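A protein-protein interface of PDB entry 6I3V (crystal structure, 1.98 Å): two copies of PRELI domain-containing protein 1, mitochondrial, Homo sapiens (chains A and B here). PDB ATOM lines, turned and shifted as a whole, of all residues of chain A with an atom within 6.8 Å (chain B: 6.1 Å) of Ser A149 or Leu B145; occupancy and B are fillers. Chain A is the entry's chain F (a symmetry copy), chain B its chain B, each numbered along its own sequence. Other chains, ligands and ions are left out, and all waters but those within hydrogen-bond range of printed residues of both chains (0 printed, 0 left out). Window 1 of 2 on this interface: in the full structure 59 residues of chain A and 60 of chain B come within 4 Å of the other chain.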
ATOM      1  N   LEU A  78      18.941  25.389  15.233  1.00  0.00           N
ATOM      2  CA  LEU A  78      18.410  24.284  16.004  1.00  0.00           C
ATOM      3  C   LEU A  78      19.009  24.239  17.398  1.00  0.00           C
ATOM      4  O   LEU A  78      18.323  23.846  18.350  1.00  0.00           O
ATOM      5  CB  LEU A  78      18.652  22.965  15.273  1.00  0.00           C
ATOM      6  CG  LEU A  78      17.601  22.461  14.267  1.00  0.00           C
ATOM      7  CD1 LEU A  78      17.218  23.482  13.205  1.00  0.00           C
ATOM      8  CD2 LEU A  78      18.096  21.203  13.587  1.00  0.00           C
ATOM      9  N   SER A 144      23.228  11.724  20.514  1.00  0.00           N
ATOM     10  CA  SER A 144      22.096  11.410  21.377  1.00  0.00           C
ATOM     11  C   SER A 144      20.762  11.898  20.810  1.00  0.00           C
ATOM     12  O   SER A 144      19.701  11.553  21.380  1.00  0.00           O
ATOM     13  CB  SER A 144      22.349  12.004  22.756  1.00  0.00           C
ATOM     14  OG  SER A 144      21.849  13.321  22.727  1.00  0.00           O
ATOM     15  N   LEU A 145      20.774  12.662  19.702  1.00  0.00           N
ATOM     16  CA  LEU A 145      19.518  13.068  19.064  1.00  0.00           C
ATOM     17  C   LEU A 145      18.696  11.888  18.552  1.00  0.00           C
ATOM     18  O   LEU A 145      17.467  11.993  18.441  1.00  0.00           O
ATOM     19  CB  LEU A 145      19.778  14.038  17.923  1.00  0.00           C
ATOM     20  CG  LEU A 145      20.532  15.237  18.475  1.00  0.00           C
ATOM     21  CD1 LEU A 145      21.081  16.104  17.338  1.00  0.00           C
ATOM     22  CD2 LEU A 145      19.673  16.053  19.421  1.00  0.00           C
ATOM     23  N   PHE A 146      19.328  10.768  18.230  1.00  0.00           N
ATOM     24  CA  PHE A 146      18.547   9.614  17.831  1.00  0.00           C
ATOM     25  C   PHE A 146      17.685   9.122  18.993  1.00  0.00           C
ATOM     26  O   PHE A 146      16.514   8.808  18.797  1.00  0.00           O
ATOM     27  CB  PHE A 146      19.457   8.496  17.315  1.00  0.00           C
ATOM     28  CG  PHE A 146      20.080   8.798  15.981  1.00  0.00           C
ATOM     29  CD1 PHE A 146      19.327   8.724  14.808  1.00  0.00           C
ATOM     30  CD2 PHE A 146      21.415   9.166  15.894  1.00  0.00           C
ATOM     31  CE1 PHE A 146      19.903   8.997  13.553  1.00  0.00           C
ATOM     32  CE2 PHE A 146      22.006   9.443  14.633  1.00  0.00           C
ATOM     33  CZ  PHE A 146      21.234   9.362  13.471  1.00  0.00           C
ATOM     34  N   GLY A 147      18.269   9.048  20.198  1.00  0.00           N
ATOM     35  CA  GLY A 147      17.537   8.638  21.383  1.00  0.00           C
ATOM     36  C   GLY A 147      16.469   9.635  21.776  1.00  0.00           C
ATOM     37  O   GLY A 147      15.408   9.238  22.265  1.00  0.00           O
ATOM     38  N   VAL A 148      16.729  10.929  21.550  1.00  0.00           N
ATOM     39  CA  VAL A 148      15.718  11.964  21.710  1.00  0.00           C
ATOM     40  C   VAL A 148      14.579  11.772  20.714  1.00  0.00           C
ATOM     41  O   VAL A 148      13.411  11.839  21.098  1.00  0.00           O
ATOM     42  CB  VAL A 148      16.353  13.358  21.584  1.00  0.00           C
ATOM     43  CG1 VAL A 148      15.231  14.415  21.557  1.00  0.00           C
ATOM     44  CG2 VAL A 148      17.315  13.604  22.754  1.00  0.00           C
ATOM     45  N   SER A 149      14.886  11.484  19.434  1.00  0.00           N
ATOM     46  CA  SER A 149      13.840  11.289  18.448  1.00  0.00           C
ATOM     47  C   SER A 149      12.932  10.144  18.871  1.00  0.00           C
ATOM     48  O   SER A 149      11.689  10.246  18.776  1.00  0.00           O
ATOM     49  CB  SER A 149      14.438  10.996  17.050  1.00  0.00           C
ATOM     50  OG  SER A 149      15.280  12.079  16.601  1.00  0.00           O
ATOM     51  N   ARG A 150      13.540   9.037  19.320  1.00  0.00           N
ATOM     52  CA  ARG A 150      12.743   7.903  19.763  1.00  0.00           C
ATOM     53  C   ARG A 150      11.936   8.249  21.011  1.00  0.00           C
ATOM     54  O   ARG A 150      10.808   7.781  21.160  1.00  0.00           O
ATOM     55  CB  ARG A 150      13.626   6.686  20.036  1.00  0.00           C
ATOM     56  N   ALA A 151      12.492   9.040  21.923  1.00  0.00           N
ATOM     57  CA  ALA A 151      11.741   9.366  23.131  1.00  0.00           C
ATOM     58  C   ALA A 151      10.537  10.256  22.825  1.00  0.00           C
ATOM     59  O   ALA A 151       9.475  10.115  23.471  1.00  0.00           O
ATOM     60  CB  ALA A 151      12.637  10.033  24.170  1.00  0.00           C
ATOM     61  N   VAL A 152      10.710  11.215  21.912  1.00  0.00           N
ATOM     62  CA  VAL A 152       9.622  12.080  21.477  1.00  0.00           C
ATOM     63  C   VAL A 152       8.514  11.236  20.851  1.00  0.00           C
ATOM     64  O   VAL A 152       7.312  11.397  21.147  1.00  0.00           O
ATOM     65  CB  VAL A 152      10.127  13.120  20.458  1.00  0.00           C
ATOM     66  CG1 VAL A 152       8.857  13.768  19.731  1.00  0.00           C
ATOM     67  CG2 VAL A 152      11.056  14.195  21.066  1.00  0.00           C
ATOM     68  N   GLN A 153       8.921  10.319  19.968  1.00  0.00           N
ATOM     69  CA  GLN A 153       7.988   9.409  19.343  1.00  0.00           C
ATOM     70  C   GLN A 153       7.248   8.556  20.373  1.00  0.00           C
ATOM     71  O   GLN A 153       6.044   8.338  20.233  1.00  0.00           O
ATOM     72  CB  GLN A 153       8.743   8.530  18.373  1.00  0.00           C
ATOM     73  CG  GLN A 153       7.905   7.761  17.466  1.00  0.00           C
ATOM     74  CD  GLN A 153       8.788   7.110  16.394  1.00  0.00           C
ATOM     75  OE1 GLN A 153       9.699   6.383  16.741  1.00  0.00           O
ATOM     76  NE2 GLN A 153       8.483   7.341  15.132  1.00  0.00           N
ATOM     77  N   GLU A 154       7.954   8.045  21.386  1.00  0.00           N
ATOM     78  CA  GLU A 154       7.310   7.240  22.419  1.00  0.00           C
ATOM     79  C   GLU A 154       6.334   8.058  23.263  1.00  0.00           C
ATOM     80  O   GLU A 154       5.262   7.547  23.648  1.00  0.00           O
ATOM     81  CB  GLU A 154       8.356   6.587  23.323  1.00  0.00           C
ATOM     82  CG  GLU A 154       9.150   5.461  22.659  1.00  0.00           C
ATOM     83  CD  GLU A 154       8.256   4.393  22.006  1.00  0.00           C
ATOM     84  OE1 GLU A 154       7.180   4.059  22.565  1.00  0.00           O
ATOM     85  OE2 GLU A 154       8.614   3.905  20.909  1.00  0.00           O
ATOM     86  N   PHE B  79      12.817  21.393  24.303  1.00  0.00           N
ATOM     87  CA  PHE B  79      12.055  22.083  23.265  1.00  0.00           C
ATOM     88  C   PHE B  79      11.385  23.328  23.843  1.00  0.00           C
ATOM     89  O   PHE B  79      10.152  23.444  23.823  1.00  0.00           O
ATOM     90  CB  PHE B  79      11.029  21.124  22.642  1.00  0.00           C
ATOM     91  CG  PHE B  79      11.647  19.878  22.134  1.00  0.00           C
ATOM     92  CD1 PHE B  79      12.496  19.918  21.024  1.00  0.00           C
ATOM     93  CD2 PHE B  79      11.448  18.673  22.770  1.00  0.00           C
ATOM     94  CE1 PHE B  79      13.132  18.771  20.559  1.00  0.00           C
ATOM     95  CE2 PHE B  79      12.080  17.502  22.295  1.00  0.00           C
ATOM     96  CZ  PHE B  79      12.934  17.565  21.195  1.00  0.00           C
ATOM     97  N   ARG B 113       7.454  20.149  13.283  1.00  0.00           N
ATOM     98  CA  ARG B 113       8.864  19.747  13.296  1.00  0.00           C
ATOM     99  C   ARG B 113       9.155  18.780  14.440  1.00  0.00           C
ATOM    100  O   ARG B 113       9.988  17.864  14.310  1.00  0.00           O
ATOM    101  CB  ARG B 113       9.771  20.988  13.408  1.00  0.00           C
ATOM    102  CG  ARG B 113       9.464  22.047  12.388  1.00  0.00           C
ATOM    103  CD  ARG B 113      10.255  21.828  11.104  1.00  0.00           C
ATOM    104  NE  ARG B 113      11.628  22.356  11.201  1.00  0.00           N
ATOM    105  CZ  ARG B 113      12.739  21.606  11.258  1.00  0.00           C
ATOM    106  NH1 ARG B 113      12.669  20.272  11.215  1.00  0.00           N
ATOM    107  NH2 ARG B 113      13.932  22.194  11.347  1.00  0.00           N
ATOM    108  N   LEU B 114       8.495  18.973  15.567  1.00  0.00           N
ATOM    109  CA  LEU B 114       8.729  18.120  16.714  1.00  0.00           C
ATOM    110  C   LEU B 114       8.095  16.744  16.517  1.00  0.00           C
ATOM    111  O   LEU B 114       8.732  15.706  16.734  1.00  0.00           O
ATOM    112  CB  LEU B 114       8.161  18.815  17.956  1.00  0.00           C
ATOM    113  CG  LEU B 114       8.247  18.103  19.295  1.00  0.00           C
ATOM    114  CD1 LEU B 114       9.724  17.665  19.552  1.00  0.00           C
ATOM    115  CD2 LEU B 114       7.824  19.091  20.341  1.00  0.00           C
ATOM    116  N   SER B 143       8.492  11.859  13.529  1.00  0.00           N
ATOM    117  CA  SER B 143       9.177  13.050  14.034  1.00  0.00           C
ATOM    118  C   SER B 143      10.292  13.450  13.065  1.00  0.00           C
ATOM    119  O   SER B 143      11.150  12.617  12.756  1.00  0.00           O
ATOM    120  CB  SER B 143       9.777  12.766  15.429  1.00  0.00           C
ATOM    121  OG  SER B 143      10.607  13.875  15.829  1.00  0.00           O
ATOM    122  N   SER B 144      10.302  14.701  12.617  1.00  0.00           N
ATOM    123  CA  SER B 144      11.395  15.133  11.757  1.00  0.00           C
ATOM    124  C   SER B 144      12.755  15.120  12.475  1.00  0.00           C
ATOM    125  O   SER B 144      13.815  15.302  11.814  1.00  0.00           O
ATOM    126  CB  SER B 144      11.050  16.505  11.181  1.00  0.00           C
ATOM    127  OG  SER B 144      11.362  17.543  12.098  1.00  0.00           O
ATOM    128  N   LEU B 145      12.763  14.876  13.786  1.00  0.00           N
ATOM    129  CA  LEU B 145      14.014  14.831  14.515  1.00  0.00           C
ATOM    130  C   LEU B 145      14.912  13.676  14.070  1.00  0.00           C
ATOM    131  O   LEU B 145      16.116  13.746  14.297  1.00  0.00           O
ATOM    132  CB  LEU B 145      13.797  14.744  16.014  1.00  0.00           C
ATOM    133  CG  LEU B 145      13.142  15.984  16.624  1.00  0.00           C
ATOM    134  CD1 LEU B 145      12.642  15.738  18.004  1.00  0.00           C
ATOM    135  CD2 LEU B 145      14.237  17.061  16.680  1.00  0.00           C
ATOM    136  N   PHE B 146      14.360  12.597  13.521  1.00  0.00           N
ATOM    137  CA  PHE B 146      15.215  11.539  12.979  1.00  0.00           C
ATOM    138  C   PHE B 146      16.053  12.066  11.820  1.00  0.00           C
ATOM    139  O   PHE B 146      17.268  11.774  11.716  1.00  0.00           O
ATOM    140  CB  PHE B 146      14.342  10.368  12.525  1.00  0.00           C
ATOM    141  CG  PHE B 146      13.714   9.586  13.662  1.00  0.00           C
ATOM    142  CD1 PHE B 146      14.456   8.651  14.384  1.00  0.00           C
ATOM    143  CD2 PHE B 146      12.347   9.726  13.969  1.00  0.00           C
ATOM    144  CE1 PHE B 146      13.864   7.887  15.407  1.00  0.00           C
ATOM    145  CE2 PHE B 146      11.784   8.992  14.998  1.00  0.00           C
ATOM    146  CZ  PHE B 146      12.560   8.060  15.699  1.00  0.00           C
ATOM    147  N   GLY B 147      15.434  12.855  10.930  1.00  0.00           N
ATOM    148  CA  GLY B 147      16.216  13.496   9.873  1.00  0.00           C
ATOM    149  C   GLY B 147      17.235  14.498  10.409  1.00  0.00           C
ATOM    150  O   GLY B 147      18.340  14.628   9.862  1.00  0.00           O
ATOM    151  N   VAL B 148      16.893  15.212  11.486  1.00  0.00           N
ATOM    152  CA  VAL B 148      17.865  16.125  12.096  1.00  0.00           C
ATOM    153  C   VAL B 148      19.057  15.352  12.690  1.00  0.00           C
ATOM    154  O   VAL B 148      20.235  15.713  12.490  1.00  0.00           O
ATOM    155  CB  VAL B 148      17.171  16.991  13.150  1.00  0.00           C
ATOM    156  CG1 VAL B 148      18.194  17.722  13.974  1.00  0.00           C
ATOM    157  CG2 VAL B 148      16.080  17.974  12.497  1.00  0.00           C
ATOM    158  N   SER B 149      18.786  14.277  13.424  1.00  0.00           N
ATOM    159  CA  SER B 149      19.883  13.452  13.924  1.00  0.00           C
ATOM    160  C   SER B 149      20.819  12.986  12.798  1.00  0.00           C
ATOM    161  O   SER B 149      22.047  12.985  12.970  1.00  0.00           O
ATOM    162  CB  SER B 149      19.321  12.241  14.649  1.00  0.00           C
ATOM    163  OG  SER B 149      18.228  12.727  15.467  1.00  0.00           O
ATOM    164  N   ARG B 150      20.261  12.547  11.670  1.00  0.00           N
ATOM    165  CA  ARG B 150      21.108  12.119  10.551  1.00  0.00           C
ATOM    166  C   ARG B 150      21.905  13.286   9.977  1.00  0.00           C
ATOM    167  O   ARG B 150      23.088  13.112   9.635  1.00  0.00           O
ATOM    168  CB  ARG B 150      20.284  11.450   9.447  1.00  0.00           C
ATOM    169  CG  ARG B 150      19.748  10.033   9.819  1.00  0.00           C
ATOM    170  CD  ARG B 150      19.086   9.261   8.643  1.00  0.00           C
ATOM    171  NE  ARG B 150      17.919   9.947   8.073  1.00  0.00           N
ATOM    172  CZ  ARG B 150      16.636   9.740   8.423  1.00  0.00           C
ATOM    173  NH1 ARG B 150      16.303   8.842   9.355  1.00  0.00           N
ATOM    174  NH2 ARG B 150      15.676  10.437   7.824  1.00  0.00           N
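Of the printed residues of chain B, Ser A149 touches Leu B145, Phe B146 and Ser B149. Of the printed residues of chain A, Arg B113 touches Leu A78. Printed residues of chain B within 4 Å of Gln A153: Phe B146 (3.5 Å). Printed residues of chain A within 4 Å of Phe B146: Ser A149, Arg A150 and Gln A153. Printed residues of chain A within 4 Å of Phe B79: Val A148 and Val A152. The nearest residue of chain B that does not touch Ser A149 is Ser B143 (4.6 Å). The nearest residue of chain A that does not touch Leu B145 is Val A148 (4.6 Å).
O of Leu B145 is in hydrogen-bond range of OG of Ser A149. The backbone NH of Phe B146 is in hydrogen-bond range of the side-chain hydroxyl of Ser A149 (3.3 Å). The side-chain hydroxyl of Ser B149 lies within hydrogen-bond range of the backbone carbonyl oxygen of Leu A145 (3.2 Å). The side-chain hydroxyl (OG) of Ser B149 lies within hydrogen-bond range of the side-chain hydroxyl (OG) of Ser A149 (3.2 Å).
O of Arg B113 sits at hydrogen-bond distance from OG of Ser B144. The side-chain hydroxyl of Ser B143 lies within hydrogen-bond range of the backbone carbonyl oxygen of Leu B114 (2.8 Å). The side-chain hydroxyl (OG) of Ser B143 lies close to the backbone NH (N) of Leu B145, 3.1 Å away. The backbone carbonyl oxygen (O) of Leu B145 sits at hydrogen-bond distance from the side-chain hydroxyl (OG) of Ser B149, 2.6 Å away. The backbone carbonyl oxygen (O) of Leu A145 lies within hydrogen-bond range of the side-chain hydroxyl (OG) of Ser A149.
Among the printed residues, merely in contact across the chains: Leu A78 with Arg B113 (3.99 Å), Leu A78 with Val B148 (3.5 Å), Phe A146 with Ser B149 (3.5 Å), Phe A146 with Arg B150 (3.8 Å), Val A148 with Phe B79 (3.9 Å), Arg A150 with Phe B146 (3.9 Å), Val A152 with Phe B79 (3.7 Å), Val A152 with Leu B114 (3.6 Å), Val A152 with Leu B145 (3.8 Å) and Gln A153 with Phe B146 (3.5 Å).
Of the 12 printed residues of chain A, 8 touch a printed residue of chain B. Hydrophobic or aromatic side chains of chain B within 4 Å of the printed part of chain A: Phe B79, Leu B114, Leu B145, Phe B146 and Val B148. Among the printed residues, 14 pairs touch across the chains. Among the printed residues, no Asp or Glu carboxylate lies within 4 Å of a Lys or Arg side-chain nitrogen of the other chain.
Leu A145 touches Ser B149, and with the chains exchanged Ser A149 touches Leu B145. Phe A146 touches Ser B149, and with the chains exchanged Ser A149 touches Phe B146. Phe A146 touches Arg B150, and with the chains exchanged Arg A150 touches Phe B146. Ser A149 touches its own counterpart, Ser B149. Of the 14 pairs that touch across the chains among the printed residues, 7 have their exchanged pair printed and touching as well.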
